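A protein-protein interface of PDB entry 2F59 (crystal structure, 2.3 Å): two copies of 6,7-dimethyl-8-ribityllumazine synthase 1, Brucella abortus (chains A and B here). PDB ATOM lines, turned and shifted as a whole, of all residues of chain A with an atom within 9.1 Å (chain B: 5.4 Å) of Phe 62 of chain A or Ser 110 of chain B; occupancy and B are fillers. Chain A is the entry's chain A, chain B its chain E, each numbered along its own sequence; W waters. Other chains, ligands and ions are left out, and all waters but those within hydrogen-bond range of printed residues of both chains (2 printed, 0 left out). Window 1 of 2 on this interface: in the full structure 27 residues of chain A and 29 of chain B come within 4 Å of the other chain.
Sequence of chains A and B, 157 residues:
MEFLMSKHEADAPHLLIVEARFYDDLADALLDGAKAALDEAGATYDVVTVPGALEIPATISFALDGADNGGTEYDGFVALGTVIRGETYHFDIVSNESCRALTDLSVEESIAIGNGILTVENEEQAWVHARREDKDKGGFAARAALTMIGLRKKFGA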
ATOM      1  N   LEU A  16     -17.921  -1.287  -7.075  1.00  0.00           N
ATOM      2  CA  LEU A  16     -18.426  -0.267  -7.976  1.00  0.00           C
ATOM      3  C   LEU A  16     -19.798  -0.771  -8.395  1.00  0.00           C
ATOM      4  O   LEU A  16     -19.931  -1.886  -8.919  1.00  0.00           O
ATOM      5  CB  LEU A  16     -17.558  -0.100  -9.224  1.00  0.00           C
ATOM      6  CG  LEU A  16     -18.220   0.798 -10.289  1.00  0.00           C
ATOM      7  CD1 LEU A  16     -18.530   2.169  -9.688  1.00  0.00           C
ATOM      8  CD2 LEU A  16     -17.319   0.934 -11.518  1.00  0.00           C
ATOM      9  N   VAL A  18     -22.676  -0.388 -10.862  1.00  0.00           N
ATOM     10  CA  VAL A  18     -22.939   0.183 -12.171  1.00  0.00           C
ATOM     11  C   VAL A  18     -24.401  -0.061 -12.472  1.00  0.00           C
ATOM     12  O   VAL A  18     -24.821  -1.189 -12.740  1.00  0.00           O
ATOM     13  CB  VAL A  18     -22.067  -0.469 -13.253  1.00  0.00           C
ATOM     14  CG1 VAL A  18     -22.273   0.250 -14.581  1.00  0.00           C
ATOM     15  CG2 VAL A  18     -20.597  -0.425 -12.822  1.00  0.00           C
ATOM     16  N   VAL A  48     -22.112   4.416 -10.201  1.00  0.00           N
ATOM     17  CA  VAL A  48     -21.989   5.122 -11.457  1.00  0.00           C
ATOM     18  C   VAL A  48     -23.258   4.760 -12.212  1.00  0.00           C
ATOM     19  O   VAL A  48     -23.713   3.614 -12.180  1.00  0.00           O
ATOM     20  CB  VAL A  48     -20.709   4.687 -12.231  1.00  0.00           C
ATOM     21  CG1 VAL A  48     -20.818   3.239 -12.666  1.00  0.00           C
ATOM     22  CG2 VAL A  48     -20.492   5.604 -13.416  1.00  0.00           C
ATOM     23  N   VAL A  50     -25.516   4.638 -15.811  1.00  0.00           N
ATOM     24  CA  VAL A  50     -25.463   4.634 -17.262  1.00  0.00           C
ATOM     25  C   VAL A  50     -26.897   4.633 -17.775  1.00  0.00           C
ATOM     26  O   VAL A  50     -27.817   4.237 -17.064  1.00  0.00           O
ATOM     27  CB  VAL A  50     -24.689   3.419 -17.800  1.00  0.00           C
ATOM     28  CG1 VAL A  50     -23.239   3.510 -17.358  1.00  0.00           C
ATOM     29  CG2 VAL A  50     -25.329   2.120 -17.314  1.00  0.00           C
ATOM     30  N   GLU A  55     -24.691  -0.328 -21.814  1.00  0.00           N
ATOM     31  CA  GLU A  55     -23.395   0.258 -21.490  1.00  0.00           C
ATOM     32  C   GLU A  55     -22.784  -0.164 -20.155  1.00  0.00           C
ATOM     33  O   GLU A  55     -21.747   0.354 -19.765  1.00  0.00           O
ATOM     34  CB  GLU A  55     -23.391   1.797 -21.605  1.00  0.00           C
ATOM     35  CG  GLU A  55     -24.671   2.513 -21.357  1.00  0.00           C
ATOM     36  CD  GLU A  55     -25.618   2.447 -22.528  1.00  0.00           C
ATOM     37  OE1 GLU A  55     -25.199   2.057 -23.636  1.00  0.00           O
ATOM     38  OE2 GLU A  55     -26.792   2.799 -22.335  1.00  0.00           O
ATOM     39  N   ILE A  56     -23.394  -1.129 -19.475  1.00  0.00           N
ATOM     40  CA  ILE A  56     -22.850  -1.580 -18.200  1.00  0.00           C
ATOM     41  C   ILE A  56     -21.489  -2.274 -18.359  1.00  0.00           C
ATOM     42  O   ILE A  56     -20.542  -1.964 -17.632  1.00  0.00           O
ATOM     43  CB  ILE A  56     -23.835  -2.529 -17.465  1.00  0.00           C
ATOM     44  CG1 ILE A  56     -25.038  -1.728 -16.949  1.00  0.00           C
ATOM     45  CG2 ILE A  56     -23.137  -3.214 -16.303  1.00  0.00           C
ATOM     46  CD1 ILE A  56     -26.071  -2.571 -16.229  1.00  0.00           C
ATOM     47  N   PRO A  57     -21.374  -3.230 -19.303  1.00  0.00           N
ATOM     48  CA  PRO A  57     -20.071  -3.885 -19.450  1.00  0.00           C
ATOM     49  C   PRO A  57     -18.923  -2.922 -19.769  1.00  0.00           C
ATOM     50  O   PRO A  57     -17.875  -2.971 -19.121  1.00  0.00           O
ATOM     51  CB  PRO A  57     -20.314  -4.939 -20.542  1.00  0.00           C
ATOM     52  CG  PRO A  57     -21.616  -4.536 -21.175  1.00  0.00           C
ATOM     53  CD  PRO A  57     -22.410  -3.932 -20.081  1.00  0.00           C
ATOM     54  N   ALA A  58     -19.123  -2.037 -20.744  1.00  0.00           N
ATOM     55  CA  ALA A  58     -18.085  -1.070 -21.104  1.00  0.00           C
ATOM     56  C   ALA A  58     -17.692  -0.209 -19.892  1.00  0.00           C
ATOM     57  O   ALA A  58     -16.524   0.138 -19.703  1.00  0.00           O
ATOM     58  CB  ALA A  58     -18.573  -0.180 -22.240  1.00  0.00           C
ATOM     59  N   THR A  59     -18.677   0.138 -19.075  1.00  0.00           N
ATOM     60  CA  THR A  59     -18.415   0.946 -17.900  1.00  0.00           C
ATOM     61  C   THR A  59     -17.461   0.208 -16.963  1.00  0.00           C
ATOM     62  O   THR A  59     -16.506   0.791 -16.453  1.00  0.00           O
ATOM     63  CB  THR A  59     -19.722   1.281 -17.172  1.00  0.00           C
ATOM     64  OG1 THR A  59     -20.563   2.026 -18.062  1.00  0.00           O
ATOM     65  CG2 THR A  59     -19.449   2.116 -15.912  1.00  0.00           C
ATOM     66  N   ILE A  60     -17.710  -1.076 -16.736  1.00  0.00           N
ATOM     67  CA  ILE A  60     -16.822  -1.840 -15.876  1.00  0.00           C
ATOM     68  C   ILE A  60     -15.446  -1.857 -16.538  1.00  0.00           C
ATOM     69  O   ILE A  60     -14.411  -1.790 -15.868  1.00  0.00           O
ATOM     70  CB  ILE A  60     -17.340  -3.271 -15.680  1.00  0.00           C
ATOM     71  CG1 ILE A  60     -18.599  -3.227 -14.803  1.00  0.00           C
ATOM     72  CG2 ILE A  60     -16.256  -4.145 -15.042  1.00  0.00           C
ATOM     73  CD1 ILE A  60     -19.270  -4.572 -14.614  1.00  0.00           C
ATOM     74  N   SER A  61     -15.445  -1.922 -17.864  1.00  0.00           N
ATOM     75  CA  SER A  61     -14.205  -1.919 -18.613  1.00  0.00           C
ATOM     76  C   SER A  61     -13.441  -0.618 -18.335  1.00  0.00           C
ATOM     77  O   SER A  61     -12.229  -0.642 -18.111  1.00  0.00           O
ATOM     78  CB  SER A  61     -14.491  -2.056 -20.105  1.00  0.00           C
ATOM     79  OG  SER A  61     -13.291  -2.316 -20.804  1.00  0.00           O
ATOM     80  N   PHE A  62     -14.157   0.506 -18.341  1.00  0.00           N
ATOM     81  CA  PHE A  62     -13.568   1.811 -18.068  1.00  0.00           C
ATOM     82  C   PHE A  62     -12.922   1.814 -16.688  1.00  0.00           C
ATOM     83  O   PHE A  62     -11.801   2.287 -16.508  1.00  0.00           O
ATOM     84  CB  PHE A  62     -14.641   2.910 -18.083  1.00  0.00           C
ATOM     85  CG  PHE A  62     -15.269   3.150 -19.427  1.00  0.00           C
ATOM     86  CD1 PHE A  62     -16.409   3.938 -19.530  1.00  0.00           C
ATOM     87  CD2 PHE A  62     -14.730   2.604 -20.579  1.00  0.00           C
ATOM     88  CE1 PHE A  62     -16.999   4.178 -20.763  1.00  0.00           C
ATOM     89  CE2 PHE A  62     -15.317   2.840 -21.821  1.00  0.00           C
ATOM     90  CZ  PHE A  62     -16.452   3.628 -21.912  1.00  0.00           C
ATOM     91  N   ALA A  63     -13.658   1.300 -15.710  1.00  0.00           N
ATOM     92  CA  ALA A  63     -13.184   1.247 -14.340  1.00  0.00           C
ATOM     93  C   ALA A  63     -11.934   0.404 -14.225  1.00  0.00           C
ATOM     94  O   ALA A  63     -11.038   0.723 -13.449  1.00  0.00           O
ATOM     95  CB  ALA A  63     -14.265   0.688 -13.437  1.00  0.00           C
ATOM     96  N   LEU A  64     -11.872  -0.677 -14.991  1.00  0.00           N
ATOM     97  CA  LEU A  64     -10.711  -1.553 -14.936  1.00  0.00           C
ATOM     98  C   LEU A  64      -9.486  -0.871 -15.523  1.00  0.00           C
ATOM     99  O   LEU A  64      -8.388  -0.981 -14.976  1.00  0.00           O
ATOM    100  CB  LEU A  64     -10.993  -2.862 -15.672  1.00  0.00           C
ATOM    101  CG  LEU A  64     -11.955  -3.807 -14.943  1.00  0.00           C
ATOM    102  CD1 LEU A  64     -12.189  -5.060 -15.788  1.00  0.00           C
ATOM    103  CD2 LEU A  64     -11.370  -4.179 -13.580  1.00  0.00           C
ATOM    104  N   ASP A  65      -9.667  -0.165 -16.636  1.00  0.00           N
ATOM    105  CA  ASP A  65      -8.551   0.531 -17.256  1.00  0.00           C
ATOM    106  C   ASP A  65      -8.198   1.757 -16.434  1.00  0.00           C
ATOM    107  O   ASP A  65      -7.039   2.162 -16.367  1.00  0.00           O
ATOM    108  CB  ASP A  65      -8.893   0.939 -18.685  1.00  0.00           C
ATOM    109  CG  ASP A  65      -9.070  -0.252 -19.594  1.00  0.00           C
ATOM    110  OD1 ASP A  65      -8.518  -1.328 -19.277  1.00  0.00           O
ATOM    111  OD2 ASP A  65      -9.749  -0.114 -20.627  1.00  0.00           O
ATOM    112  N   GLY A  66      -9.208   2.344 -15.808  1.00  0.00           N
ATOM    113  CA  GLY A  66      -8.965   3.508 -14.982  1.00  0.00           C
ATOM    114  C   GLY A  66      -8.098   3.094 -13.809  1.00  0.00           C
ATOM    115  O   GLY A  66      -7.174   3.809 -13.419  1.00  0.00           O
ATOM    116  N   ALA A  67      -8.393   1.922 -13.252  1.00  0.00           N
ATOM    117  CA  ALA A  67      -7.646   1.402 -12.117  1.00  0.00           C
ATOM    118  C   ALA A  67      -6.212   1.075 -12.527  1.00  0.00           C
ATOM    119  O   ALA A  67      -5.284   1.253 -11.738  1.00  0.00           O
ATOM    120  CB  ALA A  67      -8.332   0.161 -11.559  1.00  0.00           C
ATOM    121  N   ASP A  68      -6.032   0.595 -13.756  1.00  0.00           N
ATOM    122  CA  ASP A  68      -4.696   0.277 -14.242  1.00  0.00           C
ATOM    123  C   ASP A  68      -3.926   1.559 -14.541  1.00  0.00           C
ATOM    124  O   ASP A  68      -2.751   1.527 -14.896  1.00  0.00           O
ATOM    125  CB  ASP A  68      -4.757  -0.606 -15.493  1.00  0.00           C
ATOM    126  CG  ASP A  68      -5.094  -2.052 -15.166  1.00  0.00           C
ATOM    127  OD1 ASP A  68      -4.818  -2.483 -14.024  1.00  0.00           O
ATOM    128  OD2 ASP A  68      -5.618  -2.763 -16.052  1.00  0.00           O
ATOM    129  N   ASN A  69      -4.606   2.690 -14.401  1.00  0.00           N
ATOM    130  CA  ASN A  69      -3.992   3.989 -14.615  1.00  0.00           C
ATOM    131  C   ASN A  69      -4.012   4.730 -13.285  1.00  0.00           C
ATOM    132  O   ASN A  69      -4.205   5.944 -13.232  1.00  0.00           O
ATOM    133  CB  ASN A  69      -4.757   4.778 -15.678  1.00  0.00           C
ATOM    134  CG  ASN A  69      -4.559   4.213 -17.070  1.00  0.00           C
ATOM    135  OD1 ASN A  69      -5.276   4.575 -18.004  1.00  0.00           O
ATOM    136  ND2 ASN A  69      -3.575   3.324 -17.219  1.00  0.00           N
ATOM    137  N   GLY A  71      -6.225   4.708 -11.044  1.00  0.00           N
ATOM    138  CA  GLY A  71      -7.542   5.117 -10.583  1.00  0.00           C
ATOM    139  C   GLY A  71      -8.076   4.235  -9.467  1.00  0.00           C
ATOM    140  O   GLY A  71      -7.380   3.349  -8.978  1.00  0.00           O
ATOM    141  N   THR A  72      -9.319   4.467  -9.065  1.00  0.00           N
ATOM    142  CA  THR A  72      -9.918   3.677  -7.997  1.00  0.00           C
ATOM    143  C   THR A  72      -9.912   2.178  -8.300  1.00  0.00           C
ATOM    144  O   THR A  72     -10.356   1.729  -9.359  1.00  0.00           O
ATOM    145  CB  THR A  72     -11.361   4.137  -7.719  1.00  0.00           C
ATOM    146  OG1 THR A  72     -11.348   5.520  -7.338  1.00  0.00           O
ATOM    147  CG2 THR A  72     -11.986   3.311  -6.602  1.00  0.00           C
ATOM    148  N   TYR A  74     -11.400  -1.287  -7.646  1.00  0.00           N
ATOM    149  CA  TYR A  74     -12.586  -1.915  -7.084  1.00  0.00           C
ATOM    150  C   TYR A  74     -12.379  -3.402  -6.850  1.00  0.00           C
ATOM    151  O   TYR A  74     -11.757  -4.093  -7.654  1.00  0.00           O
ATOM    152  CB  TYR A  74     -13.800  -1.692  -7.992  1.00  0.00           C
ATOM    153  CG  TYR A  74     -14.216  -0.247  -8.090  1.00  0.00           C
ATOM    154  CD1 TYR A  74     -13.813   0.543  -9.164  1.00  0.00           C
ATOM    155  CD2 TYR A  74     -14.991   0.343  -7.090  1.00  0.00           C
ATOM    156  CE1 TYR A  74     -14.171   1.884  -9.241  1.00  0.00           C
ATOM    157  CE2 TYR A  74     -15.356   1.680  -7.160  1.00  0.00           C
ATOM    158  CZ  TYR A  74     -14.939   2.442  -8.239  1.00  0.00           C
ATOM    159  OH  TYR A  74     -15.273   3.767  -8.307  1.00  0.00           O
ATOM    160  N   PHE A  77     -17.825  -5.815  -8.676  1.00  0.00           N
ATOM    161  CA  PHE A  77     -18.812  -5.010  -9.365  1.00  0.00           C
ATOM    162  C   PHE A  77     -20.217  -5.554  -9.230  1.00  0.00           C
ATOM    163  O   PHE A  77     -20.442  -6.765  -9.179  1.00  0.00           O
ATOM    164  CB  PHE A  77     -18.461  -4.895 -10.845  1.00  0.00           C
ATOM    165  CG  PHE A  77     -17.099  -4.343 -11.090  1.00  0.00           C
ATOM    166  CD1 PHE A  77     -15.975  -5.154 -10.960  1.00  0.00           C
ATOM    167  CD2 PHE A  77     -16.929  -3.005 -11.403  1.00  0.00           C
ATOM    168  CE1 PHE A  77     -14.702  -4.634 -11.137  1.00  0.00           C
ATOM    169  CE2 PHE A  77     -15.658  -2.477 -11.580  1.00  0.00           C
ATOM    170  CZ  PHE A  77     -14.543  -3.291 -11.446  1.00  0.00           C
ATOM    171  N   LEU A 105     -16.597 -10.845 -19.273  1.00  0.00           N
ATOM    172  CA  LEU A 105     -15.750  -9.918 -18.565  1.00  0.00           C
ATOM    173  C   LEU A 105     -15.283 -10.584 -17.267  1.00  0.00           C
ATOM    174  O   LEU A 105     -14.094 -10.559 -16.934  1.00  0.00           O
ATOM    175  CB  LEU A 105     -16.551  -8.646 -18.292  1.00  0.00           C
ATOM    176  CG  LEU A 105     -15.894  -7.316 -17.946  1.00  0.00           C
ATOM    177  CD1 LEU A 105     -14.737  -7.001 -18.888  1.00  0.00           C
ATOM    178  CD2 LEU A 105     -16.964  -6.237 -18.035  1.00  0.00           C
ATOM    179  N   GLU A 109     -11.269 -11.138 -17.331  1.00  0.00           N
ATOM    180  CA  GLU A 109     -10.557 -10.318 -16.364  1.00  0.00           C
ATOM    181  C   GLU A 109     -10.475 -10.944 -14.987  1.00  0.00           C
ATOM    182  O   GLU A 109      -9.850 -10.381 -14.092  1.00  0.00           O
ATOM    183  CB  GLU A 109     -11.244  -8.960 -16.231  1.00  0.00           C
ATOM    184  CG  GLU A 109     -11.405  -8.213 -17.530  1.00  0.00           C
ATOM    185  CD  GLU A 109     -10.077  -7.927 -18.188  1.00  0.00           C
ATOM    186  OE1 GLU A 109      -9.160  -7.464 -17.478  1.00  0.00           O
ATOM    187  OE2 GLU A 109      -9.948  -8.159 -19.408  1.00  0.00           O
ATOM    188  N   LEU B 105     -17.118  -4.722 -28.689  1.00  0.00           N
ATOM    189  CA  LEU B 105     -16.249  -3.639 -29.094  1.00  0.00           C
ATOM    190  C   LEU B 105     -16.109  -2.602 -27.983  1.00  0.00           C
ATOM    191  O   LEU B 105     -14.993  -2.220 -27.616  1.00  0.00           O
ATOM    192  CB  LEU B 105     -16.817  -3.003 -30.361  1.00  0.00           C
ATOM    193  CG  LEU B 105     -15.862  -2.303 -31.314  1.00  0.00           C
ATOM    194  CD1 LEU B 105     -14.663  -3.200 -31.615  1.00  0.00           C
ATOM    195  CD2 LEU B 105     -16.625  -1.954 -32.594  1.00  0.00           C
ATOM    196  N   SER B 106     -17.230  -2.163 -27.424  1.00  0.00           N
ATOM    197  CA  SER B 106     -17.175  -1.158 -26.372  1.00  0.00           C
ATOM    198  C   SER B 106     -16.340  -1.667 -25.208  1.00  0.00           C
ATOM    199  O   SER B 106     -15.572  -0.915 -24.614  1.00  0.00           O
ATOM    200  CB  SER B 106     -18.583  -0.788 -25.891  1.00  0.00           C
ATOM    201  OG  SER B 106     -19.176  -1.837 -25.142  1.00  0.00           O
ATOM    202  N   VAL B 107     -16.476  -2.950 -24.896  1.00  0.00           N
ATOM    203  CA  VAL B 107     -15.725  -3.537 -23.797  1.00  0.00           C
ATOM    204  C   VAL B 107     -14.268  -3.779 -24.156  1.00  0.00           C
ATOM    205  O   VAL B 107     -13.363  -3.291 -23.483  1.00  0.00           O
ATOM    206  CB  VAL B 107     -16.350  -4.874 -23.353  1.00  0.00           C
ATOM    207  CG1 VAL B 107     -15.397  -5.612 -22.406  1.00  0.00           C
ATOM    208  CG2 VAL B 107     -17.676  -4.608 -22.668  1.00  0.00           C
ATOM    209  N   GLU B 108     -14.051  -4.532 -25.228  1.00  0.00           N
ATOM    210  CA  GLU B 108     -12.712  -4.868 -25.685  1.00  0.00           C
ATOM    211  C   GLU B 108     -11.857  -3.636 -25.942  1.00  0.00           C
ATOM    212  O   GLU B 108     -10.704  -3.586 -25.535  1.00  0.00           O
ATOM    213  CB  GLU B 108     -12.801  -5.727 -26.953  1.00  0.00           C
ATOM    214  CG  GLU B 108     -12.454  -7.206 -26.743  1.00  0.00           C
ATOM    215  CD  GLU B 108     -13.151  -8.134 -27.742  1.00  0.00           C
ATOM    216  OE1 GLU B 108     -14.327  -8.504 -27.501  1.00  0.00           O
ATOM    217  OE2 GLU B 108     -12.529  -8.486 -28.771  1.00  0.00           O
ATOM    218  N   GLU B 109     -12.427  -2.636 -26.602  1.00  0.00           N
ATOM    219  CA  GLU B 109     -11.677  -1.427 -26.913  1.00  0.00           C
ATOM    220  C   GLU B 109     -11.860  -0.314 -25.889  1.00  0.00           C
ATOM    221  O   GLU B 109     -11.199   0.716 -25.976  1.00  0.00           O
ATOM    222  CB  GLU B 109     -12.077  -0.904 -28.294  1.00  0.00           C
ATOM    223  CG  GLU B 109     -11.821  -1.877 -29.424  1.00  0.00           C
ATOM    224  CD  GLU B 109     -10.356  -2.249 -29.535  1.00  0.00           C
ATOM    225  OE1 GLU B 109      -9.514  -1.330 -29.499  1.00  0.00           O
ATOM    226  OE2 GLU B 109     -10.046  -3.455 -29.667  1.00  0.00           O
ATOM    227  N   SER B 110     -12.752  -0.521 -24.926  1.00  0.00           N
ATOM    228  CA  SER B 110     -13.020   0.493 -23.911  1.00  0.00           C
ATOM    229  C   SER B 110     -13.363   1.828 -24.556  1.00  0.00           C
ATOM    230  O   SER B 110     -12.716   2.847 -24.306  1.00  0.00           O
ATOM    231  CB  SER B 110     -11.816   0.657 -22.983  1.00  0.00           C
ATOM    232  OG  SER B 110     -11.700  -0.481 -22.147  1.00  0.00           O
ATOM    233  N   ILE B 111     -14.387   1.810 -25.397  1.00  0.00           N
ATOM    234  CA  ILE B 111     -14.816   3.018 -26.071  1.00  0.00           C
ATOM    235  C   ILE B 111     -16.264   3.350 -25.748  1.00  0.00           C
ATOM    236  O   ILE B 111     -17.040   2.485 -25.325  1.00  0.00           O
ATOM    237  CB  ILE B 111     -14.653   2.882 -27.597  1.00  0.00           C
ATOM    238  CG1 ILE B 111     -15.382   1.622 -28.090  1.00  0.00           C
ATOM    239  CG2 ILE B 111     -13.166   2.852 -27.949  1.00  0.00           C
ATOM    240  CD1 ILE B 111     -15.275   1.389 -29.598  1.00  0.00           C
ATOM    241  N   ALA B 112     -16.614   4.613 -25.959  1.00  0.00           N
ATOM    242  CA  ALA B 112     -17.952   5.099 -25.696  1.00  0.00           C
ATOM    243  C   ALA B 112     -18.812   4.892 -26.930  1.00  0.00           C
ATOM    244  O   ALA B 112     -18.566   5.480 -27.982  1.00  0.00           O
ATOM    245  CB  ALA B 112     -17.906   6.581 -25.324  1.00  0.00           C
ATOM    246  N   MET B 148     -21.212   8.098 -21.785  1.00  0.00           N
ATOM    247  CA  MET B 148     -20.108   7.159 -21.731  1.00  0.00           C
ATOM    248  C   MET B 148     -18.783   7.859 -21.943  1.00  0.00           C
ATOM    249  O   MET B 148     -17.774   7.460 -21.358  1.00  0.00           O
ATOM    250  CB  MET B 148     -20.305   6.046 -22.756  1.00  0.00           C
ATOM    251  CG  MET B 148     -21.489   5.154 -22.433  1.00  0.00           C
ATOM    252  SD  MET B 148     -21.303   4.405 -20.792  1.00  0.00           S
ATOM    253  CE  MET B 148     -20.273   2.964 -21.184  1.00  0.00           C
ATOM    254  N   LEU B 151     -17.956   9.213 -18.643  1.00  0.00           N
ATOM    255  CA  LEU B 151     -17.540   8.192 -17.693  1.00  0.00           C
ATOM    256  C   LEU B 151     -16.152   7.677 -18.032  1.00  0.00           C
ATOM    257  O   LEU B 151     -15.356   7.369 -17.146  1.00  0.00           O
ATOM    258  CB  LEU B 151     -18.537   7.035 -17.672  1.00  0.00           C
ATOM    259  CG  LEU B 151     -19.903   7.404 -17.086  1.00  0.00           C
ATOM    260  CD1 LEU B 151     -20.771   6.156 -16.998  1.00  0.00           C
ATOM    261  CD2 LEU B 151     -19.728   8.025 -15.698  1.00  0.00           C
ATOM    262  N   ARG B 152     -15.860   7.584 -19.320  1.00  0.00           N
ATOM    263  CA  ARG B 152     -14.561   7.105 -19.747  1.00  0.00           C
ATOM    264  C   ARG B 152     -13.511   8.040 -19.149  1.00  0.00           C
ATOM    265  O   ARG B 152     -12.470   7.597 -18.648  1.00  0.00           O
ATOM    266  CB  ARG B 152     -14.477   7.103 -21.273  1.00  0.00           C
ATOM    267  CG  ARG B 152     -13.292   6.346 -21.834  1.00  0.00           C
ATOM    268  CD  ARG B 152     -13.275   6.446 -23.346  1.00  0.00           C
ATOM    269  NE  ARG B 152     -12.023   5.964 -23.922  1.00  0.00           N
ATOM    270  CZ  ARG B 152     -11.657   6.174 -25.184  1.00  0.00           C
ATOM    271  NH1 ARG B 152     -12.448   6.857 -26.003  1.00  0.00           N
ATOM    272  NH2 ARG B 152     -10.498   5.704 -25.631  1.00  0.00           N
ATOM    273  N   PHE B 155     -13.344   7.840 -14.996  1.00  0.00           N
ATOM    274  CA  PHE B 155     -12.556   6.718 -14.502  1.00  0.00           C
ATOM    275  C   PHE B 155     -11.105   6.820 -14.981  1.00  0.00           C
ATOM    276  O   PHE B 155     -10.230   6.073 -14.536  1.00  0.00           O
ATOM    277  CB  PHE B 155     -13.154   5.379 -14.965  1.00  0.00           C
ATOM    278  CG  PHE B 155     -14.417   4.989 -14.246  1.00  0.00           C
ATOM    279  CD1 PHE B 155     -15.655   5.075 -14.883  1.00  0.00           C
ATOM    280  CD2 PHE B 155     -14.371   4.547 -12.926  1.00  0.00           C
ATOM    281  CE1 PHE B 155     -16.829   4.730 -14.218  1.00  0.00           C
ATOM    282  CE2 PHE B 155     -15.543   4.198 -12.245  1.00  0.00           C
ATOM    283  CZ  PHE B 155     -16.775   4.290 -12.892  1.00  0.00           C
ATOM    284  N   GLY B 156     -10.853   7.757 -15.885  1.00  0.00           N
ATOM    285  CA  GLY B 156      -9.515   7.918 -16.408  1.00  0.00           C
ATOM    286  C   GLY B 156      -9.112   6.685 -17.187  1.00  0.00           C
ATOM    287  O   GLY B 156      -7.982   6.215 -17.077  1.00  0.00           O
ATOM    288  N   ALA B 157     -10.039   6.154 -17.975  1.00  0.00           N
ATOM    289  CA  ALA B 157      -9.752   4.969 -18.774  1.00  0.00           C
ATOM    290  C   ALA B 157      -8.779   5.319 -19.898  1.00  0.00           C
ATOM    291  O   ALA B 157      -8.584   6.531 -20.150  1.00  0.00           O
ATOM    292  CB  ALA B 157     -11.044   4.402 -19.354  1.00  0.00           C
ATOM    293  OXT ALA B 157      -8.235   4.379 -20.521  1.00  0.00           O
HETATM  294  O   HOH W   1     -10.410   5.398 -12.089  1.00  0.00           O
HETATM  295  O   HOH W   2     -20.864  -2.179 -22.758  1.00  0.00           O
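The side-chain hydroxyl (OG1) of Thr 59 of chain A lies close to the side-chain sulfur (SD) of Met 148 of chain B (3.7 Å). OD2 of Asp 65 of chain A sits at hydrogen-bond distance from OG of Ser 110 of chain B (2.5 Å). The side-chain amide oxygen (OD1) of Asn 69 of chain A lies close to the backbone carbonyl oxygen (O) of Gly 156 of chain B. The side-chain hydroxyl (OG) of Ser 61 of chain A sits at hydrogen-bond distance from the backbone carbonyl oxygen (O) of Val 107 of chain B, 2.9 Å away. The side-chain hydroxyl (OG) of Ser 61 of chain A lies within hydrogen-bond range of the side-chain hydroxyl (OG) of Ser 110 of chain B (2.8 Å).
O of Ser 110 of chain B is in hydrogen-bond range of NE of Arg 152 of chain B (3.2 Å). The backbone NH of Ile 111 of chain B sits at hydrogen-bond distance from the backbone carbonyl oxygen of Ser 106 of chain B (3.1 Å).
Among the printed residues, pairs that only touch across the chains: Leu 16 of chain A with Phe 155 of chain B, Val 48 of chain A with Leu 151 of chain B, Val 48 of chain A with Phe 155 of chain B, Val 50 of chain A with Leu 151 of chain B, Glu 55 of chain A with Met 148 of chain B, Pro 57 of chain A with Val 107 of chain B, Ala 58 of chain A with Ser 106 of chain B, Ala 58 of chain A with Val 107 of chain B, Ala 58 of chain A with Met 148 of chain B, Phe 62 of chain A with Ser 110 of chain B, Phe 62 of chain A with Ile 111 of chain B, Phe 62 of chain A with Met 148 of chain B, Phe 62 of chain A with Arg 152 of chain B, Phe 62 of chain A with Phe 155 of chain B, Phe 62 of chain A with Ala 157 of chain B, Ala 63 of chain A with Phe 155 of chain B, Asp 65 of chain A with Ala 157 of chain B, Gly 66 of chain A with Phe 155 of chain B, Gly 66 of chain A with Gly 156 of chain B, Gly 66 of chain A with Ala 157 of chain B, Asn 69 of chain A with Ala 157 of chain B, Tyr 74 of chain A with Phe 155 of chain B and Leu 105 of chain A with Val 107 of chain B.
Phe 62 of chain A touches just these residues of chain B: Ser 110, Ile 111, Met 148, Arg 152, Phe 155 and Ala 157. Ser 110 of chain B touches just these residues of chain A: Ser 61, Phe 62 and Asp 65. Of the printed residues of chain A, Arg 152 of chain B touches Phe 62 (3.7 Å). Of the printed residues of chain B, Gly 66 of chain A touches Phe 155, Gly 156 and Ala 157. Printed residues of chain A within 4 Å of Val 107 of chain B: Pro 57 (3.4 Å), Ala 58 (3.5 Å), Ser 61 (2.9 Å) and Leu 105 (3.8 Å). The nearest residue of chain B that does not touch Phe 62 of chain A is Leu 151 of chain B (4.04 Å). The nearest printed residue of chain B that does not touch Asn 69 of chain A is Phe 155 of chain B (5.7 Å).
Hydrophobic or aromatic side chains of chain B within 4 Å of the printed part of chain A: Val 107, Met 148, Leu 151, Phe 155 and Ala 157. Printed residues of chain A that touch a printed residue of chain B: Leu 16, Val 48, Val 50, Glu 55, Pro 57, Ala 58, Thr 59, Ser 61, Phe 62, Ala 63, Asp 65, Gly 66, Asn 69, Tyr 74 and Leu 105. Hydrophobic or aromatic side chains of chain A that line the printed part of chain B: Leu 16, Val 48, Val 50, Pro 57, Ala 58, Phe 62, Ala 63, Tyr 74 and Leu 105. Among the printed residues, 28 pairs touch across the chains.
2 positions are printed for both chains. Of the 28 pairs that touch across the chains among the printed residues, none has its exchanged pair printed and touching as well.
Water W1 lies within hydrogen-bond range of O of Phe 155 of chain B (2.5 Å) and N of Thr 72 of chain A (3.3 Å). Water W2 lies within hydrogen-bond range of the backbone NH (N) of Ala 58 of chain A and the side-chain hydroxyl (OG) of Ser 106 of chain B.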
